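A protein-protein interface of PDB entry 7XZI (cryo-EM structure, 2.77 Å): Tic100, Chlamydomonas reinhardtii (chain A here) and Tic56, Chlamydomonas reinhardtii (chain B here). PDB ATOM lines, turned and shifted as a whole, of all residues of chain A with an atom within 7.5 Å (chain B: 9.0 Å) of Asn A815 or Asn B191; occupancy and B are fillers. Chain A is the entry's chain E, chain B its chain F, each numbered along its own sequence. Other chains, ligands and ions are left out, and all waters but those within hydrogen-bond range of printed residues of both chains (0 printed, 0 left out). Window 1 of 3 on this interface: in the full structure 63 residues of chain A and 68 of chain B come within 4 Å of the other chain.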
ATOM      1  N   ILE A 810      15.217 -22.913  12.521  1.00  0.00           N
ATOM      2  CA  ILE A 810      15.627 -22.362  13.812  1.00  0.00           C
ATOM      3  C   ILE A 810      17.092 -22.684  14.092  1.00  0.00           C
ATOM      4  O   ILE A 810      17.842 -21.845  14.604  1.00  0.00           O
ATOM      5  CB  ILE A 810      14.706 -22.882  14.932  1.00  0.00           C
ATOM      6  CG1 ILE A 810      13.274 -22.393  14.714  1.00  0.00           C
ATOM      7  CG2 ILE A 810      15.217 -22.444  16.293  1.00  0.00           C
ATOM      8  CD1 ILE A 810      12.309 -22.833  15.793  1.00  0.00           C
ATOM      9  N   TYR A 811      17.517 -23.905  13.761  1.00  0.00           N
ATOM     10  CA  TYR A 811      18.879 -24.341  14.053  1.00  0.00           C
ATOM     11  C   TYR A 811      19.908 -23.514  13.294  1.00  0.00           C
ATOM     12  O   TYR A 811      20.958 -23.162  13.842  1.00  0.00           O
ATOM     13  CB  TYR A 811      19.031 -25.825  13.714  1.00  0.00           C
ATOM     14  CG  TYR A 811      20.405 -26.401  13.984  1.00  0.00           C
ATOM     15  CD1 TYR A 811      20.721 -26.937  15.223  1.00  0.00           C
ATOM     16  CD2 TYR A 811      21.380 -26.423  12.994  1.00  0.00           C
ATOM     17  CE1 TYR A 811      21.970 -27.468  15.474  1.00  0.00           C
ATOM     18  CE2 TYR A 811      22.632 -26.950  13.237  1.00  0.00           C
ATOM     19  CZ  TYR A 811      22.921 -27.472  14.478  1.00  0.00           C
ATOM     20  OH  TYR A 811      24.166 -28.000  14.724  1.00  0.00           O
ATOM     21  N   ARG A 812      19.627 -23.200  12.026  1.00  0.00           N
ATOM     22  CA  ARG A 812      20.617 -22.528  11.189  1.00  0.00           C
ATOM     23  C   ARG A 812      20.965 -21.126  11.675  1.00  0.00           C
ATOM     24  O   ARG A 812      21.979 -20.572  11.240  1.00  0.00           O
ATOM     25  CB  ARG A 812      20.132 -22.453   9.740  1.00  0.00           C
ATOM     26  CG  ARG A 812      20.338 -23.730   8.946  1.00  0.00           C
ATOM     27  CD  ARG A 812      20.197 -23.479   7.452  1.00  0.00           C
ATOM     28  NE  ARG A 812      18.862 -23.022   7.094  1.00  0.00           N
ATOM     29  CZ  ARG A 812      17.874 -23.824   6.712  1.00  0.00           C
ATOM     30  NH1 ARG A 812      18.039 -25.133   6.626  1.00  0.00           N
ATOM     31  NH2 ARG A 812      16.691 -23.296   6.410  1.00  0.00           N
ATOM     32  N   MET A 813      20.155 -20.536  12.554  1.00  0.00           N
ATOM     33  CA  MET A 813      20.401 -19.173  13.006  1.00  0.00           C
ATOM     34  C   MET A 813      21.396 -19.085  14.155  1.00  0.00           C
ATOM     35  O   MET A 813      21.792 -17.973  14.521  1.00  0.00           O
ATOM     36  CB  MET A 813      19.085 -18.512  13.422  1.00  0.00           C
ATOM     37  CG  MET A 813      18.187 -18.131  12.258  1.00  0.00           C
ATOM     38  SD  MET A 813      18.921 -16.867  11.202  1.00  0.00           S
ATOM     39  CE  MET A 813      19.142 -15.531  12.376  1.00  0.00           C
ATOM     40  N   TYR A 814      21.813 -20.213  14.733  1.00  0.00           N
ATOM     41  CA  TYR A 814      22.737 -20.205  15.856  1.00  0.00           C
ATOM     42  C   TYR A 814      23.999 -21.026  15.633  1.00  0.00           C
ATOM     43  O   TYR A 814      24.928 -20.923  16.441  1.00  0.00           O
ATOM     44  CB  TYR A 814      22.038 -20.703  17.131  1.00  0.00           C
ATOM     45  CG  TYR A 814      21.014 -19.735  17.684  1.00  0.00           C
ATOM     46  CD1 TYR A 814      19.688 -19.790  17.282  1.00  0.00           C
ATOM     47  CD2 TYR A 814      21.378 -18.765  18.611  1.00  0.00           C
ATOM     48  CE1 TYR A 814      18.751 -18.908  17.784  1.00  0.00           C
ATOM     49  CE2 TYR A 814      20.448 -17.880  19.119  1.00  0.00           C
ATOM     50  CZ  TYR A 814      19.137 -17.955  18.702  1.00  0.00           C
ATOM     51  OH  TYR A 814      18.208 -17.074  19.206  1.00  0.00           O
ATOM     52  N   ASN A 815      24.068 -21.828  14.572  1.00  0.00           N
ATOM     53  CA  ASN A 815      25.233 -22.659  14.297  1.00  0.00           C
ATOM     54  C   ASN A 815      25.744 -22.356  12.898  1.00  0.00           C
ATOM     55  O   ASN A 815      24.973 -22.380  11.934  1.00  0.00           O
ATOM     56  CB  ASN A 815      24.892 -24.145  14.431  1.00  0.00           C
ATOM     57  CG  ASN A 815      24.334 -24.493  15.796  1.00  0.00           C
ATOM     58  OD1 ASN A 815      25.080 -24.806  16.722  1.00  0.00           O
ATOM     59  ND2 ASN A 815      23.014 -24.437  15.926  1.00  0.00           N
ATOM     60  N   PHE A 816      27.040 -22.077  12.788  1.00  0.00           N
ATOM     61  CA  PHE A 816      27.663 -21.696  11.531  1.00  0.00           C
ATOM     62  C   PHE A 816      28.828 -22.627  11.214  1.00  0.00           C
ATOM     63  O   PHE A 816      29.206 -23.487  12.012  1.00  0.00           O
ATOM     64  CB  PHE A 816      28.144 -20.239  11.574  1.00  0.00           C
ATOM     65  CG  PHE A 816      27.052 -19.251  11.855  1.00  0.00           C
ATOM     66  CD1 PHE A 816      26.296 -18.721  10.824  1.00  0.00           C
ATOM     67  CD2 PHE A 816      26.780 -18.853  13.152  1.00  0.00           C
ATOM     68  CE1 PHE A 816      25.289 -17.812  11.083  1.00  0.00           C
ATOM     69  CE2 PHE A 816      25.775 -17.945  13.416  1.00  0.00           C
ATOM     70  CZ  PHE A 816      25.030 -17.424  12.380  1.00  0.00           C
ATOM     71  N   ASP A 817      29.390 -22.448  10.022  1.00  0.00           N
ATOM     72  CA  ASP A 817      30.533 -23.224   9.567  1.00  0.00           C
ATOM     73  C   ASP A 817      31.801 -22.390   9.678  1.00  0.00           C
ATOM     74  O   ASP A 817      31.795 -21.190   9.393  1.00  0.00           O
ATOM     75  CB  ASP A 817      30.340 -23.688   8.122  1.00  0.00           C
ATOM     76  CG  ASP A 817      29.043 -24.442   7.922  1.00  0.00           C
ATOM     77  OD1 ASP A 817      28.602 -25.133   8.864  1.00  0.00           O
ATOM     78  OD2 ASP A 817      28.461 -24.340   6.823  1.00  0.00           O
ATOM     79  N   GLN A 826      26.579 -17.784   3.485  1.00  0.00           N
ATOM     80  CA  GLN A 826      27.552 -17.455   4.521  1.00  0.00           C
ATOM     81  C   GLN A 826      28.902 -17.089   3.919  1.00  0.00           C
ATOM     82  O   GLN A 826      29.615 -16.236   4.461  1.00  0.00           O
ATOM     83  CB  GLN A 826      27.696 -18.624   5.497  1.00  0.00           C
ATOM     84  CG  GLN A 826      28.605 -18.332   6.679  1.00  0.00           C
ATOM     85  CD  GLN A 826      28.634 -19.458   7.695  1.00  0.00           C
ATOM     86  OE1 GLN A 826      27.787 -20.351   7.677  1.00  0.00           O
ATOM     87  NE2 GLN A 826      29.615 -19.420   8.589  1.00  0.00           N
ATOM     88  N   TRP B 145      12.468 -26.367  33.300  1.00  0.00           N
ATOM     89  CA  TRP B 145      12.699 -26.377  31.864  1.00  0.00           C
ATOM     90  C   TRP B 145      11.597 -27.138  31.143  1.00  0.00           C
ATOM     91  O   TRP B 145      10.906 -27.979  31.724  1.00  0.00           O
ATOM     92  CB  TRP B 145      14.059 -27.002  31.536  1.00  0.00           C
ATOM     93  CG  TRP B 145      15.186 -26.368  32.274  1.00  0.00           C
ATOM     94  CD1 TRP B 145      15.663 -26.723  33.500  1.00  0.00           C
ATOM     95  CD2 TRP B 145      15.976 -25.255  31.841  1.00  0.00           C
ATOM     96  NE1 TRP B 145      16.706 -25.904  33.857  1.00  0.00           N
ATOM     97  CE2 TRP B 145      16.917 -24.994  32.856  1.00  0.00           C
ATOM     98  CE3 TRP B 145      15.981 -24.457  30.694  1.00  0.00           C
ATOM     99  CZ2 TRP B 145      17.854 -23.968  32.758  1.00  0.00           C
ATOM    100  CZ3 TRP B 145      16.910 -23.439  30.600  1.00  0.00           C
ATOM    101  CH2 TRP B 145      17.835 -23.203  31.625  1.00  0.00           C
ATOM    102  N   ASP B 173      18.625 -34.917  23.387  1.00  0.00           N
ATOM    103  CA  ASP B 173      20.040 -34.750  23.093  1.00  0.00           C
ATOM    104  C   ASP B 173      20.329 -33.256  22.991  1.00  0.00           C
ATOM    105  O   ASP B 173      19.501 -32.416  23.353  1.00  0.00           O
ATOM    106  CB  ASP B 173      20.427 -35.517  21.822  1.00  0.00           C
ATOM    107  CG  ASP B 173      19.665 -35.048  20.601  1.00  0.00           C
ATOM    108  OD1 ASP B 173      18.521 -34.573  20.758  1.00  0.00           O
ATOM    109  OD2 ASP B 173      20.208 -35.155  19.483  1.00  0.00           O
ATOM    110  N   GLU B 174      21.520 -32.922  22.490  1.00  0.00           N
ATOM    111  CA  GLU B 174      21.944 -31.530  22.418  1.00  0.00           C
ATOM    112  C   GLU B 174      21.192 -30.727  21.366  1.00  0.00           C
ATOM    113  O   GLU B 174      21.303 -29.497  21.361  1.00  0.00           O
ATOM    114  CB  GLU B 174      23.446 -31.461  22.142  1.00  0.00           C
ATOM    115  CG  GLU B 174      23.864 -32.140  20.852  1.00  0.00           C
ATOM    116  CD  GLU B 174      25.361 -32.097  20.634  1.00  0.00           C
ATOM    117  OE1 GLU B 174      26.074 -31.547  21.500  1.00  0.00           O
ATOM    118  OE2 GLU B 174      25.827 -32.614  19.597  1.00  0.00           O
ATOM    119  N   ASN B 175      20.441 -31.379  20.480  1.00  0.00           N
ATOM    120  CA  ASN B 175      19.705 -30.694  19.427  1.00  0.00           C
ATOM    121  C   ASN B 175      18.237 -30.472  19.768  1.00  0.00           C
ATOM    122  O   ASN B 175      17.508 -29.904  18.951  1.00  0.00           O
ATOM    123  CB  ASN B 175      19.815 -31.476  18.114  1.00  0.00           C
ATOM    124  CG  ASN B 175      21.248 -31.637  17.650  1.00  0.00           C
ATOM    125  OD1 ASN B 175      22.089 -30.769  17.879  1.00  0.00           O
ATOM    126  ND2 ASN B 175      21.535 -32.756  16.995  1.00  0.00           N
ATOM    127  N   THR B 176      17.786 -30.908  20.941  1.00  0.00           N
ATOM    128  CA  THR B 176      16.391 -30.730  21.318  1.00  0.00           C
ATOM    129  C   THR B 176      16.113 -29.269  21.657  1.00  0.00           C
ATOM    130  O   THR B 176      16.977 -28.550  22.165  1.00  0.00           O
ATOM    131  CB  THR B 176      16.043 -31.626  22.508  1.00  0.00           C
ATOM    132  OG1 THR B 176      16.529 -32.951  22.267  1.00  0.00           O
ATOM    133  CG2 THR B 176      14.537 -31.689  22.716  1.00  0.00           C
ATOM    134  N   LEU B 177      14.891 -28.829  21.366  1.00  0.00           N
ATOM    135  CA  LEU B 177      14.483 -27.455  21.630  1.00  0.00           C
ATOM    136  C   LEU B 177      13.992 -27.339  23.068  1.00  0.00           C
ATOM    137  O   LEU B 177      13.041 -28.025  23.464  1.00  0.00           O
ATOM    138  CB  LEU B 177      13.397 -27.009  20.651  1.00  0.00           C
ATOM    139  CG  LEU B 177      13.816 -26.831  19.190  1.00  0.00           C
ATOM    140  CD1 LEU B 177      12.721 -26.132  18.402  1.00  0.00           C
ATOM    141  CD2 LEU B 177      15.122 -26.060  19.091  1.00  0.00           C
ATOM    142  N   PHE B 178      14.639 -26.468  23.839  1.00  0.00           N
ATOM    143  CA  PHE B 178      14.349 -26.264  25.249  1.00  0.00           C
ATOM    144  C   PHE B 178      13.958 -24.815  25.509  1.00  0.00           C
ATOM    145  O   PHE B 178      14.264 -23.912  24.727  1.00  0.00           O
ATOM    146  CB  PHE B 178      15.555 -26.633  26.128  1.00  0.00           C
ATOM    147  CG  PHE B 178      15.625 -28.088  26.494  1.00  0.00           C
ATOM    148  CD1 PHE B 178      16.260 -28.995  25.664  1.00  0.00           C
ATOM    149  CD2 PHE B 178      15.070 -28.546  27.678  1.00  0.00           C
ATOM    150  CE1 PHE B 178      16.331 -30.332  26.002  1.00  0.00           C
ATOM    151  CE2 PHE B 178      15.139 -29.882  28.021  1.00  0.00           C
ATOM    152  CZ  PHE B 178      15.771 -30.776  27.181  1.00  0.00           C
ATOM    153  N   LEU B 183      14.856 -17.001  28.870  1.00  0.00           N
ATOM    154  CA  LEU B 183      14.820 -16.889  27.421  1.00  0.00           C
ATOM    155  C   LEU B 183      13.486 -16.319  26.954  1.00  0.00           C
ATOM    156  O   LEU B 183      12.521 -16.207  27.717  1.00  0.00           O
ATOM    157  CB  LEU B 183      15.072 -18.254  26.771  1.00  0.00           C
ATOM    158  CG  LEU B 183      16.346 -18.970  27.220  1.00  0.00           C
ATOM    159  CD1 LEU B 183      16.463 -20.334  26.566  1.00  0.00           C
ATOM    160  CD2 LEU B 183      17.576 -18.123  26.926  1.00  0.00           C
ATOM    161  N   TRP B 186      12.343 -20.611  21.907  1.00  0.00           N
ATOM    162  CA  TRP B 186      12.823 -21.974  22.088  1.00  0.00           C
ATOM    163  C   TRP B 186      14.103 -22.165  21.286  1.00  0.00           C
ATOM    164  O   TRP B 186      14.142 -21.872  20.088  1.00  0.00           O
ATOM    165  CB  TRP B 186      11.761 -22.985  21.650  1.00  0.00           C
ATOM    166  CG  TRP B 186      10.450 -22.811  22.350  1.00  0.00           C
ATOM    167  CD1 TRP B 186       9.536 -21.822  22.140  1.00  0.00           C
ATOM    168  CD2 TRP B 186       9.900 -23.652  23.373  1.00  0.00           C
ATOM    169  NE1 TRP B 186       8.455 -21.989  22.968  1.00  0.00           N
ATOM    170  CE2 TRP B 186       8.654 -23.106  23.736  1.00  0.00           C
ATOM    171  CE3 TRP B 186      10.341 -24.811  24.017  1.00  0.00           C
ATOM    172  CZ2 TRP B 186       7.843 -23.677  24.713  1.00  0.00           C
ATOM    173  CZ3 TRP B 186       9.535 -25.378  24.987  1.00  0.00           C
ATOM    174  CH2 TRP B 186       8.301 -24.811  25.326  1.00  0.00           C
ATOM    175  N   LEU B 187      15.143 -22.655  21.946  1.00  0.00           N
ATOM    176  CA  LEU B 187      16.467 -22.778  21.362  1.00  0.00           C
ATOM    177  C   LEU B 187      16.980 -24.198  21.534  1.00  0.00           C
ATOM    178  O   LEU B 187      16.514 -24.934  22.410  1.00  0.00           O
ATOM    179  CB  LEU B 187      17.449 -21.791  22.011  1.00  0.00           C
ATOM    180  CG  LEU B 187      17.051 -20.315  22.021  1.00  0.00           C
ATOM    181  CD1 LEU B 187      18.143 -19.470  22.653  1.00  0.00           C
ATOM    182  CD2 LEU B 187      16.741 -19.831  20.616  1.00  0.00           C
ATOM    183  N   PRO B 188      17.932 -24.619  20.700  1.00  0.00           N
ATOM    184  CA  PRO B 188      18.576 -25.919  20.917  1.00  0.00           C
ATOM    185  C   PRO B 188      19.289 -25.961  22.260  1.00  0.00           C
ATOM    186  O   PRO B 188      19.760 -24.943  22.770  1.00  0.00           O
ATOM    187  CB  PRO B 188      19.564 -26.024  19.750  1.00  0.00           C
ATOM    188  CG  PRO B 188      18.990 -25.143  18.696  1.00  0.00           C
ATOM    189  CD  PRO B 188      18.344 -24.004  19.427  1.00  0.00           C
ATOM    190  N   ALA B 189      19.356 -27.166  22.833  1.00  0.00           N
ATOM    191  CA  ALA B 189      19.885 -27.322  24.185  1.00  0.00           C
ATOM    192  C   ALA B 189      21.330 -26.861  24.293  1.00  0.00           C
ATOM    193  O   ALA B 189      21.719 -26.277  25.311  1.00  0.00           O
ATOM    194  CB  ALA B 189      19.763 -28.779  24.630  1.00  0.00           C
ATOM    195  N   LYS B 190      22.144 -27.111  23.267  1.00  0.00           N
ATOM    196  CA  LYS B 190      23.541 -26.702  23.321  1.00  0.00           C
ATOM    197  C   LYS B 190      23.729 -25.204  23.122  1.00  0.00           C
ATOM    198  O   LYS B 190      24.825 -24.699  23.385  1.00  0.00           O
ATOM    199  CB  LYS B 190      24.352 -27.467  22.277  1.00  0.00           C
ATOM    200  CG  LYS B 190      23.899 -27.233  20.850  1.00  0.00           C
ATOM    201  CD  LYS B 190      24.738 -28.044  19.883  1.00  0.00           C
ATOM    202  CE  LYS B 190      24.352 -27.764  18.445  1.00  0.00           C
ATOM    203  NZ  LYS B 190      25.201 -28.532  17.496  1.00  0.00           N
ATOM    204  N   ASN B 191      22.702 -24.486  22.672  1.00  0.00           N
ATOM    205  CA  ASN B 191      22.790 -23.044  22.494  1.00  0.00           C
ATOM    206  C   ASN B 191      22.348 -22.263  23.725  1.00  0.00           C
ATOM    207  O   ASN B 191      22.512 -21.039  23.751  1.00  0.00           O
ATOM    208  CB  ASN B 191      21.961 -22.606  21.279  1.00  0.00           C
ATOM    209  CG  ASN B 191      22.562 -23.071  19.964  1.00  0.00           C
ATOM    210  OD1 ASN B 191      21.907 -23.746  19.171  1.00  0.00           O
ATOM    211  ND2 ASN B 191      23.818 -22.709  19.727  1.00  0.00           N
ATOM    212  N   ILE B 192      21.804 -22.931  24.737  1.00  0.00           N
ATOM    213  CA  ILE B 192      21.537 -22.292  26.021  1.00  0.00           C
ATOM    214  C   ILE B 192      22.844 -22.213  26.796  1.00  0.00           C
ATOM    215  O   ILE B 192      23.679 -23.123  26.723  1.00  0.00           O
ATOM    216  CB  ILE B 192      20.448 -23.061  26.792  1.00  0.00           C
ATOM    217  CG1 ILE B 192      19.191 -23.196  25.930  1.00  0.00           C
ATOM    218  CG2 ILE B 192      20.113 -22.362  28.101  1.00  0.00           C
ATOM    219  CD1 ILE B 192      18.007 -23.812  26.644  1.00  0.00           C
ATOM    220  N   LYS B 193      23.031 -21.113  27.529  1.00  0.00           N
ATOM    221  CA  LYS B 193      24.336 -20.786  28.096  1.00  0.00           C
ATOM    222  C   LYS B 193      24.867 -21.902  28.990  1.00  0.00           C
ATOM    223  O   LYS B 193      25.922 -22.488  28.719  1.00  0.00           O
ATOM    224  CB  LYS B 193      24.245 -19.473  28.876  1.00  0.00           C
ATOM    225  CG  LYS B 193      25.570 -18.738  28.989  1.00  0.00           C
ATOM    226  CD  LYS B 193      26.167 -18.497  27.616  1.00  0.00           C
ATOM    227  CE  LYS B 193      27.430 -17.655  27.693  1.00  0.00           C
ATOM    228  NZ  LYS B 193      27.156 -16.284  28.204  1.00  0.00           N
ATOM    229  N   LEU B 194      24.146 -22.210  30.068  1.00  0.00           N
ATOM    230  CA  LEU B 194      24.575 -23.218  31.040  1.00  0.00           C
ATOM    231  C   LEU B 194      23.443 -24.220  31.230  1.00  0.00           C
ATOM    232  O   LEU B 194      22.654 -24.104  32.171  1.00  0.00           O
ATOM    233  CB  LEU B 194      24.965 -22.567  32.361  1.00  0.00           C
ATOM    234  CG  LEU B 194      26.036 -21.480  32.303  1.00  0.00           C
ATOM    235  CD1 LEU B 194      26.254 -20.877  33.679  1.00  0.00           C
ATOM    236  CD2 LEU B 194      27.328 -22.052  31.756  1.00  0.00           C
ATOM    237  N   LEU B 195      23.359 -25.199  30.332  1.00  0.00           N
ATOM    238  CA  LEU B 195      22.387 -26.274  30.481  1.00  0.00           C
ATOM    239  C   LEU B 195      23.064 -27.635  30.366  1.00  0.00           C
ATOM    240  O   LEU B 195      22.666 -28.593  31.035  1.00  0.00           O
ATOM    241  CB  LEU B 195      21.275 -26.141  29.442  1.00  0.00           C
ATOM    242  CG  LEU B 195      20.174 -27.196  29.512  1.00  0.00           C
ATOM    243  CD1 LEU B 195      19.548 -27.224  30.899  1.00  0.00           C
ATOM    244  CD2 LEU B 195      19.126 -26.925  28.453  1.00  0.00           C
ATOM    245  N   LEU B 196      24.079 -27.729  29.514  1.00  0.00           N
ATOM    246  CA  LEU B 196      24.833 -28.966  29.348  1.00  0.00           C
ATOM    247  C   LEU B 196      25.761 -29.223  30.533  1.00  0.00           C
ATOM    248  O   LEU B 196      25.848 -30.368  30.994  1.00  0.00           O
ATOM    249  CB  LEU B 196      25.625 -28.948  28.036  1.00  0.00           C
ATOM    250  CG  LEU B 196      24.800 -28.927  26.747  1.00  0.00           C
ATOM    251  CD1 LEU B 196      25.677 -29.168  25.525  1.00  0.00           C
ATOM    252  CD2 LEU B 196      23.682 -29.953  26.821  1.00  0.00           C
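CG2 of Ile A810 touches O of Trp B186, 3.99 Å away.
Leu B187 touches Tyr A814 (CD2 to OH, 3.4 Å).
Tyr A814 touches Asn B191.
Asn A815 touches Lys B190.
The backbone carbonyl oxygen of Tyr A811 sits at hydrogen-bond distance from the side-chain amide nitrogen of Asn A815 (3.2 Å).
O of Glu B174 sits at hydrogen-bond distance from N of Lys B190, at 3.2 Å.
N of Phe B178 lies within hydrogen-bond range of O of Leu B187 (2.8 Å).
Asn A815 touches just these residues of chain B: Lys B190 (3.5 Å) and Asn B191 (3.5 Å).
Asn B191 touches just these residues of chain A: Tyr A814 (3.7 Å) and Asn A815 (3.5 Å).
Printed residues of chain A within 4 Å of Leu B187: Tyr A814.
Of the printed residues of chain B, Tyr A811 touches Lys B190.
Printed residues of chain B within 4 Å of Tyr A814: Leu B187 (3.4 Å) and Asn B191 (3.7 Å).
Met A813 touches none of the printed residues of chain B.
The nearest residue of chain B that does not touch Asn A815 is Pro B188 (4.9 Å).
Of the 9 printed residues of chain A, 4 touch a printed residue of chain B.
Hydrophobic or aromatic side chains of chain A within 4 Å of the printed part of chain B: Ile A810, Tyr A811 and Tyr A814.
Along chain A the printed residues that touch a printed residue of chain B span positions 810 to 815.
Of the 19 printed residues of chain B, 4 touch a printed residue of chain A.
Hydrophobic or aromatic side chains of chain B within 4 Å of the printed part of chain A: Leu B187.
Among the printed residues, 6 pairs touch across the chains.
Among the printed residues, no Asp or Glu carboxylate lies within 4 Å of a Lys or Arg side-chain nitrogen of the other chain.
The side-chain hydroxyl of Tyr A811 lies within hydrogen-bond range of the side-chain amino group of Lys B190 (3.0 Å).
ND2 of Asn A815 sits at hydrogen-bond distance from OD1 of Asn B191.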
